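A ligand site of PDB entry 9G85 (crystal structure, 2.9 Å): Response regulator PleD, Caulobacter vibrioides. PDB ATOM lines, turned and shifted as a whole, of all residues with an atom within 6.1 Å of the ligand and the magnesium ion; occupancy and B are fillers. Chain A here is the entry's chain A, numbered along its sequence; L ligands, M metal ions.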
ATOM      1  N   LEU A 294      15.230  15.185  10.781  1.00  0.00           N
ATOM      2  CA  LEU A 294      16.387  15.062  11.671  1.00  0.00           C
ATOM      3  C   LEU A 294      16.003  15.367  13.118  1.00  0.00           C
ATOM      4  O   LEU A 294      16.135  14.516  14.003  1.00  0.00           O
ATOM      5  CB  LEU A 294      17.507  16.007  11.198  1.00  0.00           C
ATOM      6  CG  LEU A 294      18.767  16.077  12.054  1.00  0.00           C
ATOM      7  CD1 LEU A 294      19.652  14.853  11.847  1.00  0.00           C
ATOM      8  CD2 LEU A 294      19.545  17.350  11.768  1.00  0.00           C
ATOM      9  N   ASP A 327      19.699  31.201  17.007  1.00  0.00           N
ATOM     10  CA  ASP A 327      20.773  30.802  16.110  1.00  0.00           C
ATOM     11  C   ASP A 327      21.949  30.307  16.940  1.00  0.00           C
ATOM     12  O   ASP A 327      22.393  30.983  17.861  1.00  0.00           O
ATOM     13  CB  ASP A 327      21.209  31.960  15.210  1.00  0.00           C
ATOM     14  CG  ASP A 327      22.079  31.522  14.057  1.00  0.00           C
ATOM     15  OD1 ASP A 327      21.520  31.185  12.995  1.00  0.00           O
ATOM     16  OD2 ASP A 327      23.325  31.503  14.216  1.00  0.00           O
ATOM     17  N   ILE A 328      22.456  29.114  16.599  1.00  0.00           N
ATOM     18  CA  ILE A 328      23.561  28.519  17.352  1.00  0.00           C
ATOM     19  C   ILE A 328      24.872  29.181  16.972  1.00  0.00           C
ATOM     20  O   ILE A 328      25.169  29.372  15.780  1.00  0.00           O
ATOM     21  CB  ILE A 328      23.616  27.003  17.110  1.00  0.00           C
ATOM     22  CG1 ILE A 328      22.263  26.362  17.445  1.00  0.00           C
ATOM     23  CG2 ILE A 328      24.725  26.367  17.941  1.00  0.00           C
ATOM     24  CD1 ILE A 328      22.222  24.863  17.221  1.00  0.00           C
ATOM     25  N   ASP A 329      25.677  29.532  17.970  1.00  0.00           N
ATOM     26  CA  ASP A 329      26.935  30.236  17.747  1.00  0.00           C
ATOM     27  C   ASP A 329      28.049  29.248  17.408  1.00  0.00           C
ATOM     28  O   ASP A 329      28.213  28.234  18.099  1.00  0.00           O
ATOM     29  CB  ASP A 329      27.325  31.049  18.974  1.00  0.00           C
ATOM     30  CG  ASP A 329      26.289  32.078  19.360  1.00  0.00           C
ATOM     31  OD1 ASP A 329      25.652  32.642  18.442  1.00  0.00           O
ATOM     32  OD2 ASP A 329      26.118  32.330  20.565  1.00  0.00           O
ATOM     33  N   PHE A 330      28.785  29.545  16.341  1.00  0.00           N
ATOM     34  CA  PHE A 330      29.981  28.784  15.956  1.00  0.00           C
ATOM     35  C   PHE A 330      29.653  27.320  15.663  1.00  0.00           C
ATOM     36  O   PHE A 330      30.317  26.410  16.151  1.00  0.00           O
ATOM     37  CB  PHE A 330      31.059  28.879  17.046  1.00  0.00           C
ATOM     38  CG  PHE A 330      31.346  30.281  17.492  1.00  0.00           C
ATOM     39  CD1 PHE A 330      31.547  31.300  16.575  1.00  0.00           C
ATOM     40  CD2 PHE A 330      31.412  30.581  18.839  1.00  0.00           C
ATOM     41  CE1 PHE A 330      31.810  32.583  16.997  1.00  0.00           C
ATOM     42  CE2 PHE A 330      31.672  31.867  19.274  1.00  0.00           C
ATOM     43  CZ  PHE A 330      31.873  32.870  18.338  1.00  0.00           C
ATOM     44  N   PHE A 331      28.627  27.099  14.844  1.00  0.00           N
ATOM     45  CA  PHE A 331      28.265  25.726  14.522  1.00  0.00           C
ATOM     46  C   PHE A 331      29.237  25.100  13.533  1.00  0.00           C
ATOM     47  O   PHE A 331      29.435  23.878  13.556  1.00  0.00           O
ATOM     48  CB  PHE A 331      26.839  25.653  13.976  1.00  0.00           C
ATOM     49  CG  PHE A 331      26.231  24.281  14.080  1.00  0.00           C
ATOM     50  CD1 PHE A 331      25.570  23.887  15.239  1.00  0.00           C
ATOM     51  CD2 PHE A 331      26.366  23.369  13.045  1.00  0.00           C
ATOM     52  CE1 PHE A 331      25.032  22.616  15.344  1.00  0.00           C
ATOM     53  CE2 PHE A 331      25.820  22.103  13.139  1.00  0.00           C
ATOM     54  CZ  PHE A 331      25.148  21.728  14.298  1.00  0.00           C
ATOM     55  N   LYS A 332      29.848  25.912  12.663  1.00  0.00           N
ATOM     56  CA  LYS A 332      30.859  25.391  11.755  1.00  0.00           C
ATOM     57  C   LYS A 332      31.988  24.705  12.505  1.00  0.00           C
ATOM     58  O   LYS A 332      32.452  23.635  12.104  1.00  0.00           O
ATOM     59  CB  LYS A 332      31.418  26.518  10.877  1.00  0.00           C
ATOM     60  CG  LYS A 332      30.373  27.182   9.981  1.00  0.00           C
ATOM     61  CD  LYS A 332      30.978  28.322   9.155  1.00  0.00           C
ATOM     62  CE  LYS A 332      29.937  28.936   8.226  1.00  0.00           C
ATOM     63  N   LYS A 333      32.440  25.308  13.615  1.00  0.00           N
ATOM     64  CA  LYS A 333      33.533  24.715  14.388  1.00  0.00           C
ATOM     65  C   LYS A 333      33.168  23.343  14.914  1.00  0.00           C
ATOM     66  O   LYS A 333      34.024  22.449  15.006  1.00  0.00           O
ATOM     67  CB  LYS A 333      33.922  25.636  15.546  1.00  0.00           C
ATOM     68  CG  LYS A 333      33.783  27.126  15.260  1.00  0.00           C
ATOM     69  N   ASN A 335      31.132  21.159  13.365  1.00  0.00           N
ATOM     70  CA  ASN A 335      31.308  20.286  12.211  1.00  0.00           C
ATOM     71  C   ASN A 335      32.777  20.086  11.884  1.00  0.00           C
ATOM     72  O   ASN A 335      33.194  18.995  11.484  1.00  0.00           O
ATOM     73  CB  ASN A 335      30.572  20.865  10.999  1.00  0.00           C
ATOM     74  CG  ASN A 335      29.071  20.752  11.136  1.00  0.00           C
ATOM     75  OD1 ASN A 335      28.548  19.758  11.621  1.00  0.00           O
ATOM     76  ND2 ASN A 335      28.361  21.781  10.691  1.00  0.00           N
ATOM     77  N   ASP A 336      33.590  21.127  12.074  1.00  0.00           N
ATOM     78  CA  ASP A 336      35.021  21.030  11.767  1.00  0.00           C
ATOM     79  C   ASP A 336      35.731  20.116  12.744  1.00  0.00           C
ATOM     80  O   ASP A 336      36.496  19.234  12.335  1.00  0.00           O
ATOM     81  CB  ASP A 336      35.650  22.424  11.805  1.00  0.00           C
ATOM     82  CG  ASP A 336      35.225  23.283  10.640  1.00  0.00           C
ATOM     83  OD1 ASP A 336      34.537  22.761   9.738  1.00  0.00           O
ATOM     84  OD2 ASP A 336      35.571  24.479  10.640  1.00  0.00           O
ATOM     85  N   GLY A 339      32.970  16.584  13.206  1.00  0.00           N
ATOM     86  CA  GLY A 339      32.378  15.964  12.029  1.00  0.00           C
ATOM     87  C   GLY A 339      30.909  16.312  11.892  1.00  0.00           C
ATOM     88  O   GLY A 339      30.253  16.805  12.808  1.00  0.00           O
ATOM     89  N   HIS A 340      30.391  16.021  10.696  1.00  0.00           N
ATOM     90  CA  HIS A 340      29.028  16.404  10.375  1.00  0.00           C
ATOM     91  C   HIS A 340      28.008  15.543  11.114  1.00  0.00           C
ATOM     92  O   HIS A 340      26.905  16.014  11.408  1.00  0.00           O
ATOM     93  CB  HIS A 340      28.798  16.332   8.863  1.00  0.00           C
ATOM     94  CG  HIS A 340      27.720  17.246   8.365  1.00  0.00           C
ATOM     95  ND1 HIS A 340      26.434  16.815   8.140  1.00  0.00           N
ATOM     96  CD2 HIS A 340      27.735  18.560   8.051  1.00  0.00           C
ATOM     97  CE1 HIS A 340      25.698  17.821   7.710  1.00  0.00           C
ATOM     98  NE2 HIS A 340      26.472  18.900   7.645  1.00  0.00           N
ATOM     99  N   ASP A 341      28.351  14.290  11.410  1.00  0.00           N
ATOM    100  CA  ASP A 341      27.411  13.412  12.104  1.00  0.00           C
ATOM    101  C   ASP A 341      27.229  13.825  13.553  1.00  0.00           C
ATOM    102  O   ASP A 341      26.117  13.759  14.099  1.00  0.00           O
ATOM    103  CB  ASP A 341      27.875  11.961  12.012  1.00  0.00           C
ATOM    104  CG  ASP A 341      27.659  11.369  10.643  1.00  0.00           C
ATOM    105  OD1 ASP A 341      27.139  12.086   9.763  1.00  0.00           O
ATOM    106  OD2 ASP A 341      28.002  10.178  10.434  1.00  0.00           O
ATOM    107  N   ILE A 342      28.312  14.248  14.214  1.00  0.00           N
ATOM    108  CA  ILE A 342      28.186  14.764  15.572  1.00  0.00           C
ATOM    109  C   ILE A 342      27.420  16.080  15.563  1.00  0.00           C
ATOM    110  O   ILE A 342      26.620  16.361  16.470  1.00  0.00           O
ATOM    111  CB  ILE A 342      29.572  14.921  16.223  1.00  0.00           C
ATOM    112  CG1 ILE A 342      30.233  13.553  16.397  1.00  0.00           C
ATOM    113  CG2 ILE A 342      29.465  15.627  17.564  1.00  0.00           C
ATOM    114  CD1 ILE A 342      29.311  12.496  16.965  1.00  0.00           C
ATOM    115  N   GLY A 343      27.639  16.904  14.537  1.00  0.00           N
ATOM    116  CA  GLY A 343      26.829  18.103  14.366  1.00  0.00           C
ATOM    117  C   GLY A 343      25.347  17.786  14.322  1.00  0.00           C
ATOM    118  O   GLY A 343      24.526  18.503  14.911  1.00  0.00           O
ATOM    119  N   ASP A 344      24.976  16.709  13.620  1.00  0.00           N
ATOM    120  CA  ASP A 344      23.575  16.305  13.586  1.00  0.00           C
ATOM    121  C   ASP A 344      23.090  15.836  14.952  1.00  0.00           C
ATOM    122  O   ASP A 344      21.918  16.052  15.294  1.00  0.00           O
ATOM    123  CB  ASP A 344      23.384  15.203  12.538  1.00  0.00           C
ATOM    124  CG  ASP A 344      23.618  15.700  11.121  1.00  0.00           C
ATOM    125  OD1 ASP A 344      24.140  16.817  10.964  1.00  0.00           O
ATOM    126  OD2 ASP A 344      23.285  14.964  10.165  1.00  0.00           O
ATOM    127  N   LEU A 347      22.238  18.958  16.913  1.00  0.00           N
ATOM    128  CA  LEU A 347      20.962  19.524  16.497  1.00  0.00           C
ATOM    129  C   LEU A 347      19.784  18.748  17.091  1.00  0.00           C
ATOM    130  O   LEU A 347      18.794  19.351  17.509  1.00  0.00           O
ATOM    131  CB  LEU A 347      20.863  19.560  14.971  1.00  0.00           C
ATOM    132  CG  LEU A 347      21.748  20.562  14.235  1.00  0.00           C
ATOM    133  CD1 LEU A 347      21.530  20.433  12.739  1.00  0.00           C
ATOM    134  CD2 LEU A 347      21.473  21.983  14.684  1.00  0.00           C
ATOM    135  N   ARG A 366      12.149  24.181  13.312  1.00  0.00           N
ATOM    136  CA  ARG A 366      13.461  24.354  12.692  1.00  0.00           C
ATOM    137  C   ARG A 366      13.281  25.344  11.542  1.00  0.00           C
ATOM    138  O   ARG A 366      12.656  25.027  10.527  1.00  0.00           O
ATOM    139  CB  ARG A 366      14.017  23.025  12.200  1.00  0.00           C
ATOM    140  CG  ARG A 366      15.468  23.131  11.770  1.00  0.00           C
ATOM    141  CD  ARG A 366      15.992  21.829  11.212  1.00  0.00           C
ATOM    142  NE  ARG A 366      17.350  21.993  10.718  1.00  0.00           N
ATOM    143  CZ  ARG A 366      18.117  21.001  10.289  1.00  0.00           C
ATOM    144  NH1 ARG A 366      17.668  19.764  10.222  1.00  0.00           N
ATOM    145  NH2 ARG A 366      19.362  21.276   9.899  1.00  0.00           N
ATOM    146  N   GLY A 368      15.869  27.434   9.896  1.00  0.00           N
ATOM    147  CA  GLY A 368      16.919  27.332   8.904  1.00  0.00           C
ATOM    148  C   GLY A 368      17.738  26.073   9.121  1.00  0.00           C
ATOM    149  O   GLY A 368      17.251  25.070   9.624  1.00  0.00           O
ATOM    150  N   GLY A 369      19.006  26.149   8.721  1.00  0.00           N
ATOM    151  CA  GLY A 369      19.905  25.034   8.939  1.00  0.00           C
ATOM    152  C   GLY A 369      20.151  24.792  10.406  1.00  0.00           C
ATOM    153  O   GLY A 369      19.740  23.753  10.951  1.00  0.00           O
ATOM    154  N   GLU A 370      20.801  25.737  11.070  1.00  0.00           N
ATOM    155  CA  GLU A 370      21.009  25.690  12.507  1.00  0.00           C
ATOM    156  C   GLU A 370      20.274  26.811  13.226  1.00  0.00           C
ATOM    157  O   GLU A 370      20.653  27.216  14.327  1.00  0.00           O
ATOM    158  CB  GLU A 370      22.506  25.728  12.832  1.00  0.00           C
ATOM    159  CG  GLU A 370      23.301  26.779  12.071  1.00  0.00           C
ATOM    160  CD  GLU A 370      23.018  28.199  12.526  1.00  0.00           C
ATOM    161  OE1 GLU A 370      23.074  28.451  13.748  1.00  0.00           O
ATOM    162  OE2 GLU A 370      22.746  29.058  11.666  1.00  0.00           O
ATOM    163  N   LYS A 442      24.416  38.920  17.432  1.00  0.00           N
ATOM    164  CA  LYS A 442      25.663  38.366  16.915  1.00  0.00           C
ATOM    165  C   LYS A 442      26.767  39.416  16.875  1.00  0.00           C
ATOM    166  O   LYS A 442      27.934  39.113  17.139  1.00  0.00           O
ATOM    167  CB  LYS A 442      25.452  37.777  15.517  1.00  0.00           C
ATOM    168  CG  LYS A 442      24.487  36.618  15.436  1.00  0.00           C
ATOM    169  CD  LYS A 442      25.107  35.330  15.932  1.00  0.00           C
ATOM    170  CE  LYS A 442      24.139  34.164  15.755  1.00  0.00           C
ATOM    171  NZ  LYS A 442      24.704  32.862  16.203  1.00  0.00           N
ATOM    172  N   ARG A 446      28.452  37.217  21.586  1.00  0.00           N
ATOM    173  CA  ARG A 446      27.610  36.055  21.401  1.00  0.00           C
ATOM    174  C   ARG A 446      26.874  35.769  22.703  1.00  0.00           C
ATOM    175  O   ARG A 446      27.107  36.416  23.722  1.00  0.00           O
ATOM    176  CB  ARG A 446      28.411  34.833  20.958  1.00  0.00           C
ATOM    177  CG  ARG A 446      29.054  34.962  19.579  1.00  0.00           C
ATOM    178  CD  ARG A 446      28.009  35.060  18.476  1.00  0.00           C
ATOM    179  NE  ARG A 446      28.585  35.512  17.209  1.00  0.00           N
ATOM    180  CZ  ARG A 446      28.923  34.706  16.213  1.00  0.00           C
ATOM    181  NH1 ARG A 446      28.764  33.392  16.291  1.00  0.00           N
ATOM    182  NH2 ARG A 446      29.428  35.238  15.098  1.00  0.00           N
HETATM  183  P1  LIG L   1      27.676  30.345  12.870  1.00  0.00           P
HETATM  184  O1  LIG L   1      28.598  31.432  13.374  1.00  0.00           O
HETATM  185  O2  LIG L   1      28.293  28.979  13.122  1.00  0.00           O
HETATM  186  O3  LIG L   1      26.408  30.505  13.663  1.00  0.00           O
HETATM  187  O4  LIG L   1      27.332  30.440  11.249  1.00  0.00           O
HETATM  188  P2  LIG L   1      26.158  29.473  10.607  1.00  0.00           P
HETATM  189  O5  LIG L   1      24.884  30.263  10.349  1.00  0.00           O
HETATM  190  O6  LIG L   1      25.920  28.427  11.685  1.00  0.00           O
HETATM  191  O7  LIG L   1      26.642  28.679   9.233  1.00  0.00           O
HETATM  192  C1  LIG L   1      25.766  27.772   8.574  1.00  0.00           C
HETATM  193  C2  LIG L   1      25.945  26.382   9.159  1.00  0.00           C
HETATM  194  O8  LIG L   1      24.850  25.790   9.470  1.00  0.00           O
HETATM  195  C3  LIG L   1      26.681  25.392   8.031  1.00  0.00           C
HETATM  196  O9  LIG L   1      28.115  25.801   7.789  1.00  0.00           O
HETATM  197  C4  LIG L   1      26.587  24.280   8.526  1.00  0.00           C
HETATM  198  O10 LIG L   1      27.819  23.920   9.301  1.00  0.00           O
HETATM  199  C5  LIG L   1      25.411  24.372   9.617  1.00  0.00           C
HETATM  200  N1  LIG L   1      24.623  23.309   9.482  1.00  0.00           N
HETATM  201  C6  LIG L   1      23.551  23.870   8.885  1.00  0.00           C
HETATM  202  N2  LIG L   1      22.652  22.836   8.710  1.00  0.00           N
HETATM  203  C7  LIG L   1      23.207  21.714   9.205  1.00  0.00           C
HETATM  204  C8  LIG L   1      22.792  20.233   9.342  1.00  0.00           C
HETATM  205  O11 LIG L   1      21.723  19.885   8.942  1.00  0.00           O
HETATM  206  N3  LIG L   1      23.651  19.237   9.941  1.00  0.00           N
HETATM  207  C9  LIG L   1      24.942  19.629  10.443  1.00  0.00           C
HETATM  208  N4  LIG L   1      25.897  18.733  11.064  1.00  0.00           N
HETATM  209  N5  LIG L   1      25.344  21.020  10.301  1.00  0.00           N
HETATM  210  C10 LIG L   1      24.447  22.035   9.681  1.00  0.00           C
HETATM  211  P3  LIG L   1      29.131  24.822   6.867  1.00  0.00           P
HETATM  212  O12 LIG L   1      29.954  25.637   5.883  1.00  0.00           O
HETATM  213  O13 LIG L   1      30.063  24.104   7.808  1.00  0.00           O
HETATM  214  O14 LIG L   1      28.211  23.666   6.074  1.00  0.00           O
HETATM  215  P4  LIG L   1      28.486  22.031   6.268  1.00  0.00           P
HETATM  216  O15 LIG L   1      27.304  21.212   5.784  1.00  0.00           O
HETATM  217  O16 LIG L   1      28.716  21.788   7.746  1.00  0.00           O
HETATM  218  O17 LIG L   1      29.723  21.637   5.490  1.00  0.00           O
HETATM  219 MG    MG M   1      24.604  29.988  13.722  1.00  0.00          MG
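N of Phe 331 lies within hydrogen-bond range of O2 of the ligand (2.6 Å). OD1 of Asp 344 sits at hydrogen-bond distance from N4 of the ligand, at 2.6 Å. ND2 of Asn 335 is in hydrogen-bond range of O10 of the ligand, at 2.6 Å. The guanidinium group (NH2) of Arg 366 sits at hydrogen-bond distance from an oxygen (O11) of the ligand. O of His 340 sits at hydrogen-bond distance from N4 of the ligand, at 2.9 Å. An oxygen (O15) of the ligand lies within hydrogen-bond range of a ring nitrogen (NE2) of His 340 (3.1 Å). An oxygen (O2) of the ligand lies close to the backbone NH (N) of Phe 330 (3.3 Å). N of Lys 332 sits at hydrogen-bond distance from O2 of the ligand (3.5 Å). An oxygen (O1) of the ligand lies within salt-bridge range of the guanidinium group (NH1) of Arg 446, 3.5 Å away. The side-chain amino group (NZ) of Lys 442 lies close to an oxygen (O3) of the ligand, at 3.9 Å.
NZ of Lys 442 is in hydrogen-bond range of O of Asp 327, 3.4 Å away. The guanidinium group of Arg 366 lies within hydrogen-bond range of the backbone carbonyl oxygen of Gly 369 (2.7 Å). The guanidinium group (NE) of Arg 366 is in hydrogen-bond range of the backbone carbonyl oxygen (O) of Gly 368. The side-chain carboxylate (OD1) of Asp 329 lies within salt-bridge range of the guanidinium group (NH1) of Arg 446, at 3.9 Å. NZ of Lys 442 is in salt-bridge range of OD1 of Asp 329 (2.4 Å).
Residues that only touch the ligand: Gly 343, Leu 347 and Gly 369. Hydrophobic or aromatic side chains that line the ligand: Phe 331, His 340 and Leu 347. 15 residues have an atom within 4 Å of the ligand: Asp 327, Ile 328, Phe 330, Phe 331, Lys 332, Asn 335, His 340, Gly 343, Asp 344, Leu 347, Arg 366, Gly 369, Glu 370, Lys 442 and Arg 446.
Merely in contact with the magnesium ion: Lys 442 (3.8 Å). Four residues have an atom within 4 Å of the magnesium ion: Asp 327, Ile 328, Glu 370 and Lys 442. Along chain A the residues within 4 Å of the magnesium ion span positions 327 to 442.
The magnesium ion is bound by an oxygen (O3) of the ligand (1.9 Å), the side-chain carboxylate (OD2) of Asp 327 (2.0 Å), the side-chain carboxylate (OE1) of Glu 370 (2.2 Å) and the backbone carbonyl oxygen (O) of Ile 328 (2.2 Å). The magnesium ion has four donor atoms within binding distance.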
